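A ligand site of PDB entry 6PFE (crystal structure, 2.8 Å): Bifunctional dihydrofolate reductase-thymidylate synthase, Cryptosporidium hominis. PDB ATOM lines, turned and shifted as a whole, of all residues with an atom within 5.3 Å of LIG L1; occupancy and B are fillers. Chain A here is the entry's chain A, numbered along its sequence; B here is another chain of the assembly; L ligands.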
ATOM      1  N   ASN A 256     -20.647 -12.359 -20.217  1.00  0.00           N
ATOM      2  CA  ASN A 256     -20.192 -13.359 -19.261  1.00  0.00           C
ATOM      3  C   ASN A 256     -20.095 -14.709 -19.971  1.00  0.00           C
ATOM      4  O   ASN A 256     -20.338 -14.814 -21.171  1.00  0.00           O
ATOM      5  CB  ASN A 256     -21.109 -13.434 -18.036  1.00  0.00           C
ATOM      6  CG  ASN A 256     -22.563 -13.638 -18.404  1.00  0.00           C
ATOM      7  OD1 ASN A 256     -22.998 -14.758 -18.651  1.00  0.00           O
ATOM      8  ND2 ASN A 256     -23.319 -12.549 -18.427  1.00  0.00           N
ATOM      9  N   ARG A 257     -19.771 -15.740 -19.194  1.00  0.00           N
ATOM     10  CA  ARG A 257     -19.521 -17.068 -19.753  1.00  0.00           C
ATOM     11  C   ARG A 257     -20.753 -17.631 -20.464  1.00  0.00           C
ATOM     12  O   ARG A 257     -20.619 -18.467 -21.361  1.00  0.00           O
ATOM     13  CB  ARG A 257     -19.078 -18.024 -18.654  1.00  0.00           C
ATOM     14  CG  ARG A 257     -20.160 -18.232 -17.615  1.00  0.00           C
ATOM     15  CD  ARG A 257     -19.797 -19.259 -16.565  1.00  0.00           C
ATOM     16  NE  ARG A 257     -20.851 -19.317 -15.557  1.00  0.00           N
ATOM     17  CZ  ARG A 257     -21.991 -19.984 -15.725  1.00  0.00           C
ATOM     18  NH1 ARG A 257     -22.215 -20.637 -16.853  1.00  0.00           N
ATOM     19  NH2 ARG A 257     -22.903 -19.986 -14.757  1.00  0.00           N
ATOM     20  N   GLU A 294     -31.747 -28.501  -1.414  1.00  0.00           N
ATOM     21  CA  GLU A 294     -30.387 -28.245  -1.878  1.00  0.00           C
ATOM     22  C   GLU A 294     -29.430 -28.085  -0.699  1.00  0.00           C
ATOM     23  O   GLU A 294     -28.265 -28.498  -0.773  1.00  0.00           O
ATOM     24  CB  GLU A 294     -30.363 -26.983  -2.735  1.00  0.00           C
ATOM     25  CG  GLU A 294     -28.970 -26.620  -3.247  1.00  0.00           C
ATOM     26  CD  GLU A 294     -28.873 -25.162  -3.633  1.00  0.00           C
ATOM     27  OE1 GLU A 294     -29.498 -24.327  -2.945  1.00  0.00           O
ATOM     28  OE2 GLU A 294     -28.164 -24.853  -4.620  1.00  0.00           O
ATOM     29  N   TRP A 316     -30.227 -27.677 -10.461  1.00  0.00           N
ATOM     30  CA  TRP A 316     -28.907 -28.037 -10.967  1.00  0.00           C
ATOM     31  C   TRP A 316     -28.999 -28.867 -12.246  1.00  0.00           C
ATOM     32  O   TRP A 316     -28.060 -29.594 -12.570  1.00  0.00           O
ATOM     33  CB  TRP A 316     -28.110 -28.784  -9.898  1.00  0.00           C
ATOM     34  CG  TRP A 316     -27.573 -27.893  -8.811  1.00  0.00           C
ATOM     35  CD1 TRP A 316     -28.132 -27.670  -7.595  1.00  0.00           C
ATOM     36  CD2 TRP A 316     -26.351 -27.136  -8.844  1.00  0.00           C
ATOM     37  NE1 TRP A 316     -27.343 -26.805  -6.860  1.00  0.00           N
ATOM     38  CE2 TRP A 316     -26.247 -26.467  -7.605  1.00  0.00           C
ATOM     39  CE3 TRP A 316     -25.348 -26.953  -9.800  1.00  0.00           C
ATOM     40  CZ2 TRP A 316     -25.180 -25.623  -7.308  1.00  0.00           C
ATOM     41  CZ3 TRP A 316     -24.295 -26.111  -9.491  1.00  0.00           C
ATOM     42  CH2 TRP A 316     -24.213 -25.466  -8.254  1.00  0.00           C
ATOM     43  N   TYR A 342     -19.851 -27.466  -3.448  1.00  0.00           N
ATOM     44  CA  TYR A 342     -20.243 -27.050  -2.109  1.00  0.00           C
ATOM     45  C   TYR A 342     -20.290 -28.194  -1.113  1.00  0.00           C
ATOM     46  O   TYR A 342     -19.658 -28.131  -0.047  1.00  0.00           O
ATOM     47  CB  TYR A 342     -21.606 -26.355  -2.153  1.00  0.00           C
ATOM     48  CG  TYR A 342     -21.684 -25.218  -3.147  1.00  0.00           C
ATOM     49  CD1 TYR A 342     -21.125 -23.981  -2.856  1.00  0.00           C
ATOM     50  CD2 TYR A 342     -22.337 -25.382  -4.367  1.00  0.00           C
ATOM     51  CE1 TYR A 342     -21.214 -22.934  -3.755  1.00  0.00           C
ATOM     52  CE2 TYR A 342     -22.417 -24.339  -5.265  1.00  0.00           C
ATOM     53  CZ  TYR A 342     -21.858 -23.120  -4.958  1.00  0.00           C
ATOM     54  OH  TYR A 342     -21.942 -22.090  -5.862  1.00  0.00           O
ATOM     55  N   LEU A 399     -19.187 -26.131 -11.758  1.00  0.00           N
ATOM     56  CA  LEU A 399     -19.339 -24.700 -11.605  1.00  0.00           C
ATOM     57  C   LEU A 399     -18.573 -24.278 -10.357  1.00  0.00           C
ATOM     58  O   LEU A 399     -18.727 -24.900  -9.297  1.00  0.00           O
ATOM     59  CB  LEU A 399     -20.816 -24.309 -11.511  1.00  0.00           C
ATOM     60  CG  LEU A 399     -21.124 -22.824 -11.630  1.00  0.00           C
ATOM     61  CD1 LEU A 399     -20.717 -22.334 -13.006  1.00  0.00           C
ATOM     62  CD2 LEU A 399     -22.593 -22.558 -11.377  1.00  0.00           C
ATOM     63  N   PRO A 400     -17.714 -23.262 -10.436  1.00  0.00           N
ATOM     64  CA  PRO A 400     -17.017 -22.809  -9.231  1.00  0.00           C
ATOM     65  C   PRO A 400     -18.004 -22.297  -8.208  1.00  0.00           C
ATOM     66  O   PRO A 400     -19.098 -21.820  -8.558  1.00  0.00           O
ATOM     67  CB  PRO A 400     -16.092 -21.698  -9.754  1.00  0.00           C
ATOM     68  CG  PRO A 400     -15.900 -22.025 -11.197  1.00  0.00           C
ATOM     69  CD  PRO A 400     -17.210 -22.600 -11.650  1.00  0.00           C
ATOM     70  N   CYS A 402     -20.213 -20.143  -5.915  1.00  0.00           N
ATOM     71  CA  CYS A 402     -20.639 -18.749  -5.896  1.00  0.00           C
ATOM     72  C   CYS A 402     -20.585 -18.182  -4.484  1.00  0.00           C
ATOM     73  O   CYS A 402     -20.047 -17.090  -4.270  1.00  0.00           O
ATOM     74  CB  CYS A 402     -22.051 -18.635  -6.469  1.00  0.00           C
ATOM     75  SG  CYS A 402     -22.140 -19.184  -8.184  1.00  0.00           S
ATOM     76  N   HIS A 403     -21.163 -18.889  -3.509  1.00  0.00           N
ATOM     77  CA  HIS A 403     -20.972 -18.532  -2.099  1.00  0.00           C
ATOM     78  C   HIS A 403     -19.703 -19.240  -1.617  1.00  0.00           C
ATOM     79  O   HIS A 403     -19.724 -20.416  -1.254  1.00  0.00           O
ATOM     80  CB  HIS A 403     -22.201 -18.889  -1.262  1.00  0.00           C
ATOM     81  CG  HIS A 403     -22.849 -20.196  -1.613  1.00  0.00           C
ATOM     82  ND1 HIS A 403     -22.746 -21.316  -0.805  1.00  0.00           N
ATOM     83  CD2 HIS A 403     -23.627 -20.553  -2.661  1.00  0.00           C
ATOM     84  CE1 HIS A 403     -23.433 -22.307  -1.349  1.00  0.00           C
ATOM     85  NE2 HIS A 403     -23.974 -21.875  -2.480  1.00  0.00           N
ATOM     86  N   GLN A 422     -20.110 -13.739  -1.320  1.00  0.00           N
ATOM     87  CA  GLN A 422     -20.618 -14.300  -2.563  1.00  0.00           C
ATOM     88  C   GLN A 422     -19.921 -13.584  -3.712  1.00  0.00           C
ATOM     89  O   GLN A 422     -20.105 -12.385  -3.902  1.00  0.00           O
ATOM     90  CB  GLN A 422     -22.133 -14.146  -2.631  1.00  0.00           C
ATOM     91  CG  GLN A 422     -22.837 -14.959  -3.702  1.00  0.00           C
ATOM     92  CD  GLN A 422     -24.349 -14.859  -3.582  1.00  0.00           C
ATOM     93  OE1 GLN A 422     -24.863 -14.337  -2.586  1.00  0.00           O
ATOM     94  NE2 GLN A 422     -25.067 -15.359  -4.581  1.00  0.00           N
ATOM     95  N   ARG A 423     -19.116 -14.338  -4.481  1.00  0.00           N
ATOM     96  CA  ARG A 423     -18.336 -13.730  -5.550  1.00  0.00           C
ATOM     97  C   ARG A 423     -19.218 -13.273  -6.698  1.00  0.00           C
ATOM     98  O   ARG A 423     -18.965 -12.233  -7.322  1.00  0.00           O
ATOM     99  CB  ARG A 423     -17.273 -14.713  -6.063  1.00  0.00           C
ATOM    100  CG  ARG A 423     -17.863 -15.961  -6.699  1.00  0.00           C
ATOM    101  CD  ARG A 423     -16.852 -16.726  -7.539  1.00  0.00           C
ATOM    102  NE  ARG A 423     -17.483 -17.861  -8.214  1.00  0.00           N
ATOM    103  CZ  ARG A 423     -18.096 -17.770  -9.385  1.00  0.00           C
ATOM    104  NH1 ARG A 423     -18.162 -16.608 -10.018  1.00  0.00           N
ATOM    105  NH2 ARG A 423     -18.651 -18.841  -9.934  1.00  0.00           N
ATOM    106  N   SER A 424     -20.260 -14.037  -7.002  1.00  0.00           N
ATOM    107  CA  SER A 424     -21.143 -13.770  -8.127  1.00  0.00           C
ATOM    108  C   SER A 424     -22.561 -14.035  -7.670  1.00  0.00           C
ATOM    109  O   SER A 424     -22.851 -15.102  -7.111  1.00  0.00           O
ATOM    110  CB  SER A 424     -20.764 -14.658  -9.325  1.00  0.00           C
ATOM    111  OG  SER A 424     -21.533 -14.341 -10.477  1.00  0.00           O
ATOM    112  N   CYS A 425     -23.443 -13.066  -7.884  1.00  0.00           N
ATOM    113  CA  CYS A 425     -24.792 -13.096  -7.328  1.00  0.00           C
ATOM    114  C   CYS A 425     -25.813 -12.862  -8.441  1.00  0.00           C
ATOM    115  O   CYS A 425     -25.909 -11.754  -8.970  1.00  0.00           O
ATOM    116  CB  CYS A 425     -24.937 -12.045  -6.230  1.00  0.00           C
ATOM    117  SG  CYS A 425     -26.597 -11.896  -5.577  1.00  0.00           S
ATOM    118  N   ASP A 426     -26.555 -13.908  -8.787  1.00  0.00           N
ATOM    119  CA  ASP A 426     -27.657 -13.821  -9.732  1.00  0.00           C
ATOM    120  C   ASP A 426     -28.893 -13.317  -8.991  1.00  0.00           C
ATOM    121  O   ASP A 426     -29.680 -14.094  -8.456  1.00  0.00           O
ATOM    122  CB  ASP A 426     -27.914 -15.173 -10.387  1.00  0.00           C
ATOM    123  CG  ASP A 426     -29.117 -15.176 -11.301  1.00  0.00           C
ATOM    124  OD1 ASP A 426     -29.671 -14.093 -11.587  1.00  0.00           O
ATOM    125  OD2 ASP A 426     -29.510 -16.269 -11.748  1.00  0.00           O
ATOM    126  N   GLY A 430     -30.497 -16.829  -7.997  1.00  0.00           N
ATOM    127  CA  GLY A 430     -29.637 -17.344  -6.946  1.00  0.00           C
ATOM    128  C   GLY A 430     -29.758 -16.585  -5.641  1.00  0.00           C
ATOM    129  O   GLY A 430     -29.746 -17.177  -4.559  1.00  0.00           O
ATOM    130  N   SER A 431     -29.901 -15.261  -5.716  1.00  0.00           N
ATOM    131  CA  SER A 431     -29.872 -14.446  -4.505  1.00  0.00           C
ATOM    132  C   SER A 431     -31.016 -14.746  -3.551  1.00  0.00           C
ATOM    133  O   SER A 431     -30.751 -14.907  -2.344  1.00  0.00           O
ATOM    134  CB  SER A 431     -29.842 -12.961  -4.879  1.00  0.00           C
ATOM    135  OG  SER A 431     -29.598 -12.161  -3.738  1.00  0.00           O
ATOM    136  N   ASN A 434     -29.874 -17.873  -1.982  1.00  0.00           N
ATOM    137  CA  ASN A 434     -28.726 -17.754  -1.086  1.00  0.00           C
ATOM    138  C   ASN A 434     -29.114 -17.088   0.240  1.00  0.00           C
ATOM    139  O   ASN A 434     -28.504 -17.379   1.269  1.00  0.00           O
ATOM    140  CB  ASN A 434     -27.619 -16.951  -1.759  1.00  0.00           C
ATOM    141  CG  ASN A 434     -27.047 -17.658  -2.967  1.00  0.00           C
ATOM    142  OD1 ASN A 434     -26.933 -17.084  -4.054  1.00  0.00           O
ATOM    143  ND2 ASN A 434     -26.680 -18.922  -2.798  1.00  0.00           N
ATOM    144  N   HIS A 464     -25.317  -8.749 -10.060  1.00  0.00           N
ATOM    145  CA  HIS A 464     -25.742  -8.531 -11.435  1.00  0.00           C
ATOM    146  C   HIS A 464     -27.181  -8.990 -11.641  1.00  0.00           C
ATOM    147  O   HIS A 464     -27.751  -9.711 -10.829  1.00  0.00           O
ATOM    148  CB  HIS A 464     -24.822  -9.256 -12.426  1.00  0.00           C
ATOM    149  CG  HIS A 464     -24.715 -10.720 -12.166  1.00  0.00           C
ATOM    150  ND1 HIS A 464     -23.705 -11.272 -11.409  1.00  0.00           N
ATOM    151  CD2 HIS A 464     -25.502 -11.756 -12.546  1.00  0.00           C
ATOM    152  CE1 HIS A 464     -23.865 -12.587 -11.347  1.00  0.00           C
ATOM    153  NE2 HIS A 464     -24.949 -12.909 -12.025  1.00  0.00           N
ATOM    154  N   TYR A 466     -29.410 -10.595 -14.950  1.00  0.00           N
ATOM    155  CA  TYR A 466     -29.402 -11.063 -16.322  1.00  0.00           C
ATOM    156  C   TYR A 466     -30.447 -10.314 -17.136  1.00  0.00           C
ATOM    157  O   TYR A 466     -31.530  -9.995 -16.639  1.00  0.00           O
ATOM    158  CB  TYR A 466     -29.650 -12.566 -16.385  1.00  0.00           C
ATOM    159  CG  TYR A 466     -28.438 -13.378 -15.984  1.00  0.00           C
ATOM    160  CD1 TYR A 466     -28.200 -13.706 -14.656  1.00  0.00           C
ATOM    161  CD2 TYR A 466     -27.528 -13.815 -16.937  1.00  0.00           C
ATOM    162  CE1 TYR A 466     -27.084 -14.446 -14.289  1.00  0.00           C
ATOM    163  CE2 TYR A 466     -26.416 -14.546 -16.584  1.00  0.00           C
ATOM    164  CZ  TYR A 466     -26.192 -14.861 -15.271  1.00  0.00           C
ATOM    165  OH  TYR A 466     -25.067 -15.597 -14.948  1.00  0.00           O
ATOM    166  N   ARG B 382     -15.904 -13.359 -13.631  1.00  0.00           N
ATOM    167  CA  ARG B 382     -16.217 -13.071 -12.238  1.00  0.00           C
ATOM    168  C   ARG B 382     -15.707 -14.144 -11.278  1.00  0.00           C
ATOM    169  O   ARG B 382     -16.384 -14.515 -10.323  1.00  0.00           O
ATOM    170  CB  ARG B 382     -17.726 -12.882 -12.096  1.00  0.00           C
ATOM    171  CG  ARG B 382     -18.557 -13.773 -13.001  1.00  0.00           C
ATOM    172  CD  ARG B 382     -19.890 -13.124 -13.304  1.00  0.00           C
ATOM    173  NE  ARG B 382     -20.811 -14.056 -13.952  1.00  0.00           N
ATOM    174  CZ  ARG B 382     -22.011 -13.731 -14.419  1.00  0.00           C
ATOM    175  NH1 ARG B 382     -22.438 -12.481 -14.308  1.00  0.00           N
ATOM    176  NH2 ARG B 382     -22.784 -14.651 -14.987  1.00  0.00           N
ATOM    177  N   ARG B 383     -14.493 -14.653 -11.521  1.00  0.00           N
ATOM    178  CA  ARG B 383     -13.864 -15.639 -10.644  1.00  0.00           C
ATOM    179  C   ARG B 383     -12.448 -15.242 -10.247  1.00  0.00           C
ATOM    180  O   ARG B 383     -11.678 -16.082  -9.792  1.00  0.00           O
ATOM    181  CB  ARG B 383     -13.856 -17.022 -11.310  1.00  0.00           C
ATOM    182  CG  ARG B 383     -15.229 -17.533 -11.668  1.00  0.00           C
ATOM    183  CD  ARG B 383     -15.138 -18.708 -12.628  1.00  0.00           C
ATOM    184  NE  ARG B 383     -16.448 -19.208 -13.000  1.00  0.00           N
ATOM    185  CZ  ARG B 383     -16.652 -20.124 -13.943  1.00  0.00           C
ATOM    186  NH1 ARG B 383     -15.626 -20.629 -14.619  1.00  0.00           N
ATOM    187  NH2 ARG B 383     -17.887 -20.524 -14.223  1.00  0.00           N
HETATM  188  N1  LIG L   1     -25.321 -18.093  -8.715  1.00  0.00           N
HETATM  189  C1  LIG L   1     -25.484 -17.528  -7.492  1.00  0.00           C
HETATM  190  N2  LIG L   1     -25.581 -18.305  -6.389  1.00  0.00           N
HETATM  191  C2  LIG L   1     -25.532 -19.646  -6.466  1.00  0.00           C
HETATM  192  C3  LIG L   1     -25.369 -20.251  -7.739  1.00  0.00           C
HETATM  193  C4  LIG L   1     -25.281 -19.464  -8.825  1.00  0.00           C
HETATM  194  O1  LIG L   1     -25.556 -16.325  -7.303  1.00  0.00           O
HETATM  195  O2  LIG L   1     -25.623 -20.315  -5.453  1.00  0.00           O
HETATM  196  F1  LIG L   1     -25.299 -21.596  -7.900  1.00  0.00           F
HETATM  197  C5  LIG L   1     -25.216 -17.416 -10.027  1.00  0.00           C
HETATM  198  C6  LIG L   1     -24.352 -16.135 -10.081  1.00  0.00           C
HETATM  199  C7  LIG L   1     -23.942 -16.119 -11.569  1.00  0.00           C
HETATM  200  C8  LIG L   1     -23.669 -17.612 -11.828  1.00  0.00           C
HETATM  201  O3  LIG L   1     -25.022 -15.697 -12.397  1.00  0.00           O
HETATM  202  O4  LIG L   1     -24.561 -18.333 -10.941  1.00  0.00           O
HETATM  203  C9  LIG L   1     -22.212 -17.933 -11.512  1.00  0.00           C
HETATM  204  O5  LIG L   1     -21.545 -18.350 -12.693  1.00  0.00           O
HETATM  205  P1  LIG L   1     -20.234 -17.434 -12.845  1.00  0.00           P
HETATM  206  O6  LIG L   1     -20.433 -16.459 -14.110  1.00  0.00           O
HETATM  207  O7  LIG L   1     -20.025 -16.616 -11.636  1.00  0.00           O
HETATM  208  O8  LIG L   1     -18.945 -18.375 -13.044  1.00  0.00           O
HETATM  209  C1  LG2 L   2     -31.005 -21.471  -8.026  1.00  0.00           C
HETATM  210  C2  LG2 L   2     -32.313 -21.350  -8.464  1.00  0.00           C
HETATM  211  C3  LG2 L   2     -32.693 -21.827  -9.715  1.00  0.00           C
HETATM  212  C4  LG2 L   2     -31.730 -22.422 -10.540  1.00  0.00           C
HETATM  213  C5  LG2 L   2     -34.123 -21.665 -10.178  1.00  0.00           C
HETATM  214  C6  LG2 L   2     -36.351 -21.010  -9.093  1.00  0.00           C
HETATM  215  C7  LG2 L   2     -37.171 -23.411  -8.792  1.00  0.00           C
HETATM  216  C8  LG2 L   2     -27.570 -21.030 -10.381  1.00  0.00           C
HETATM  217  C9  LG2 L   2     -28.214 -19.716 -10.471  1.00  0.00           C
HETATM  218  C10 LG2 L   2     -27.699 -22.126  -9.506  1.00  0.00           C
HETATM  219  C11 LG2 L   2     -26.814 -23.107  -9.933  1.00  0.00           C
HETATM  220  C12 LG2 L   2     -26.620 -21.380 -11.332  1.00  0.00           C
HETATM  221  C13 LG2 L   2     -26.767 -19.434 -12.457  1.00  0.00           C
HETATM  222  C14 LG2 L   2     -36.670 -19.662  -9.185  1.00  0.00           C
HETATM  223  C15 LG2 L   2     -37.991 -19.233  -9.127  1.00  0.00           C
HETATM  224  C16 LG2 L   2     -39.017 -20.146  -8.956  1.00  0.00           C
HETATM  225  C17 LG2 L   2     -38.711 -21.495  -8.853  1.00  0.00           C
HETATM  226  C18 LG2 L   2     -37.385 -21.937  -8.907  1.00  0.00           C
HETATM  227  C19 LG2 L   2     -37.479 -17.100  -8.414  1.00  0.00           C
HETATM  228  C20 LG2 L   2     -28.630 -22.198  -8.325  1.00  0.00           C
HETATM  229  C21 LG2 L   2     -30.041 -22.081  -8.824  1.00  0.00           C
HETATM  230  C22 LG2 L   2     -30.417 -22.552 -10.088  1.00  0.00           C
HETATM  231  N1  LG2 L   2     -27.718 -19.026 -11.546  1.00  0.00           N
HETATM  232  N2  LG2 L   2     -26.210 -20.597 -12.365  1.00  0.00           N
HETATM  233  N3  LG2 L   2     -26.158 -22.644 -11.058  1.00  0.00           N
HETATM  234  N4  LG2 L   2     -26.413 -18.489 -13.513  1.00  0.00           N
HETATM  235  N5  LG2 L   2     -34.910 -21.322  -9.150  1.00  0.00           N
HETATM  236  O1  LG2 L   2     -29.065 -19.224  -9.749  1.00  0.00           O
HETATM  237  O2  LG2 L   2     -34.512 -21.831 -11.325  1.00  0.00           O
HETATM  238  O3  LG2 L   2     -38.375 -24.029  -8.606  1.00  0.00           O
HETATM  239  O4  LG2 L   2     -36.110 -24.028  -8.859  1.00  0.00           O
HETATM  240  O5  LG2 L   2     -38.266 -17.888  -9.229  1.00  0.00           O
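An oxygen (O4) of LIG L1 lies close to a nitrogen (N4) of LG2 L2 (3.2 Å).
OD1 of Asn 434 lies close to O of Gly 430. The side-chain hydroxyl (OH) of Tyr 342 lies within hydrogen-bond range of the backbone NH (N) of Cys 402 (2.6 Å). The guanidinium group of Arg 382 of chain B sits at hydrogen-bond distance from the side-chain hydroxyl of Tyr 466 (2.5 Å). The side-chain hydroxyl of Ser 431 lies close to the side-chain sulfur of Cys 425, at 3.5 Å. NE2 of Gln 422 sits at hydrogen-bond distance from O of Ser 424, 3.4 Å away. A ring nitrogen (ND1) of His 464 sits close to the guanidinium group of Arg 382 of chain B, at 3.4 Å. The guanidinium group (NH2) of Arg 423 sits at hydrogen-bond distance from the backbone carbonyl oxygen (O) of Pro 400 (3.3 Å). The side-chain amide nitrogen (NE2) of Gln 422 sits at hydrogen-bond distance from the side-chain amide oxygen (OD1) of Asn 434 (2.6 Å).
Tyr 342 touches LIG L1 (OH to F1, 3.96 Å). His 403 touches LIG L1 (CD2 to O2, 3.4 Å). CA of Cys 425 touches O1 of LIG L1 (3.3 Å). Hydrophobic or aromatic side chains within 4 Å of LIG L1: His 403, His 464 and Tyr 466. 14 residues have an atom within 4 Å of LIG L1: Arg 257, Tyr 342, Cys 402, His 403, Gln 422, Arg 423, Ser 424, Cys 425, Asp 426, Asn 434, His 464, Tyr 466, Arg 382 of chain B and Arg 383 of chain B.
The guanidinium group (NE) of Arg 257 lies within salt-bridge range of an oxygen (O6) of LIG L1 (3.2 Å). O8 of LIG L1 is in salt-bridge range of NE of Arg 383 of chain B. An oxygen (O1) of LG2 L2 lies within hydrogen-bond range of the backbone NH of Gly 430 (3.3 Å). O1 of LIG L1 lies within hydrogen-bond range of N of Asp 426. The side-chain amide nitrogen (NE2) of Gln 422 lies within hydrogen-bond range of an oxygen (O1) of LIG L1 (2.9 Å). An oxygen (O7) of LIG L1 lies within hydrogen-bond range of the side-chain hydroxyl (OG) of Ser 424, 3.0 Å away. NH1 of Arg 423 lies within salt-bridge range of O7 of LIG L1, 2.5 Å away. OH of Tyr 466 sits at hydrogen-bond distance from O3 of LIG L1. An oxygen (O6) of LIG L1 lies within salt-bridge range of the guanidinium group (NE) of Arg 382 of chain B (2.4 Å). OH of Tyr 466 lies within hydrogen-bond range of N4 of LG2 L2 (3.5 Å). A ring nitrogen (NE2) of His 464 lies within hydrogen-bond range of an oxygen (O3) of LIG L1 (2.8 Å). OD2 of Asp 426 lies within hydrogen-bond range of N1 of LG2 L2, at 3.3 Å. The side-chain amide oxygen (OD1) of Asn 434 sits at hydrogen-bond distance from a nitrogen (N2) of LIG L1 (3.0 Å). An oxygen (O4) of LIG L1 sits close to the side-chain sulfur (SG) of Cys 402 (3.8 Å).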
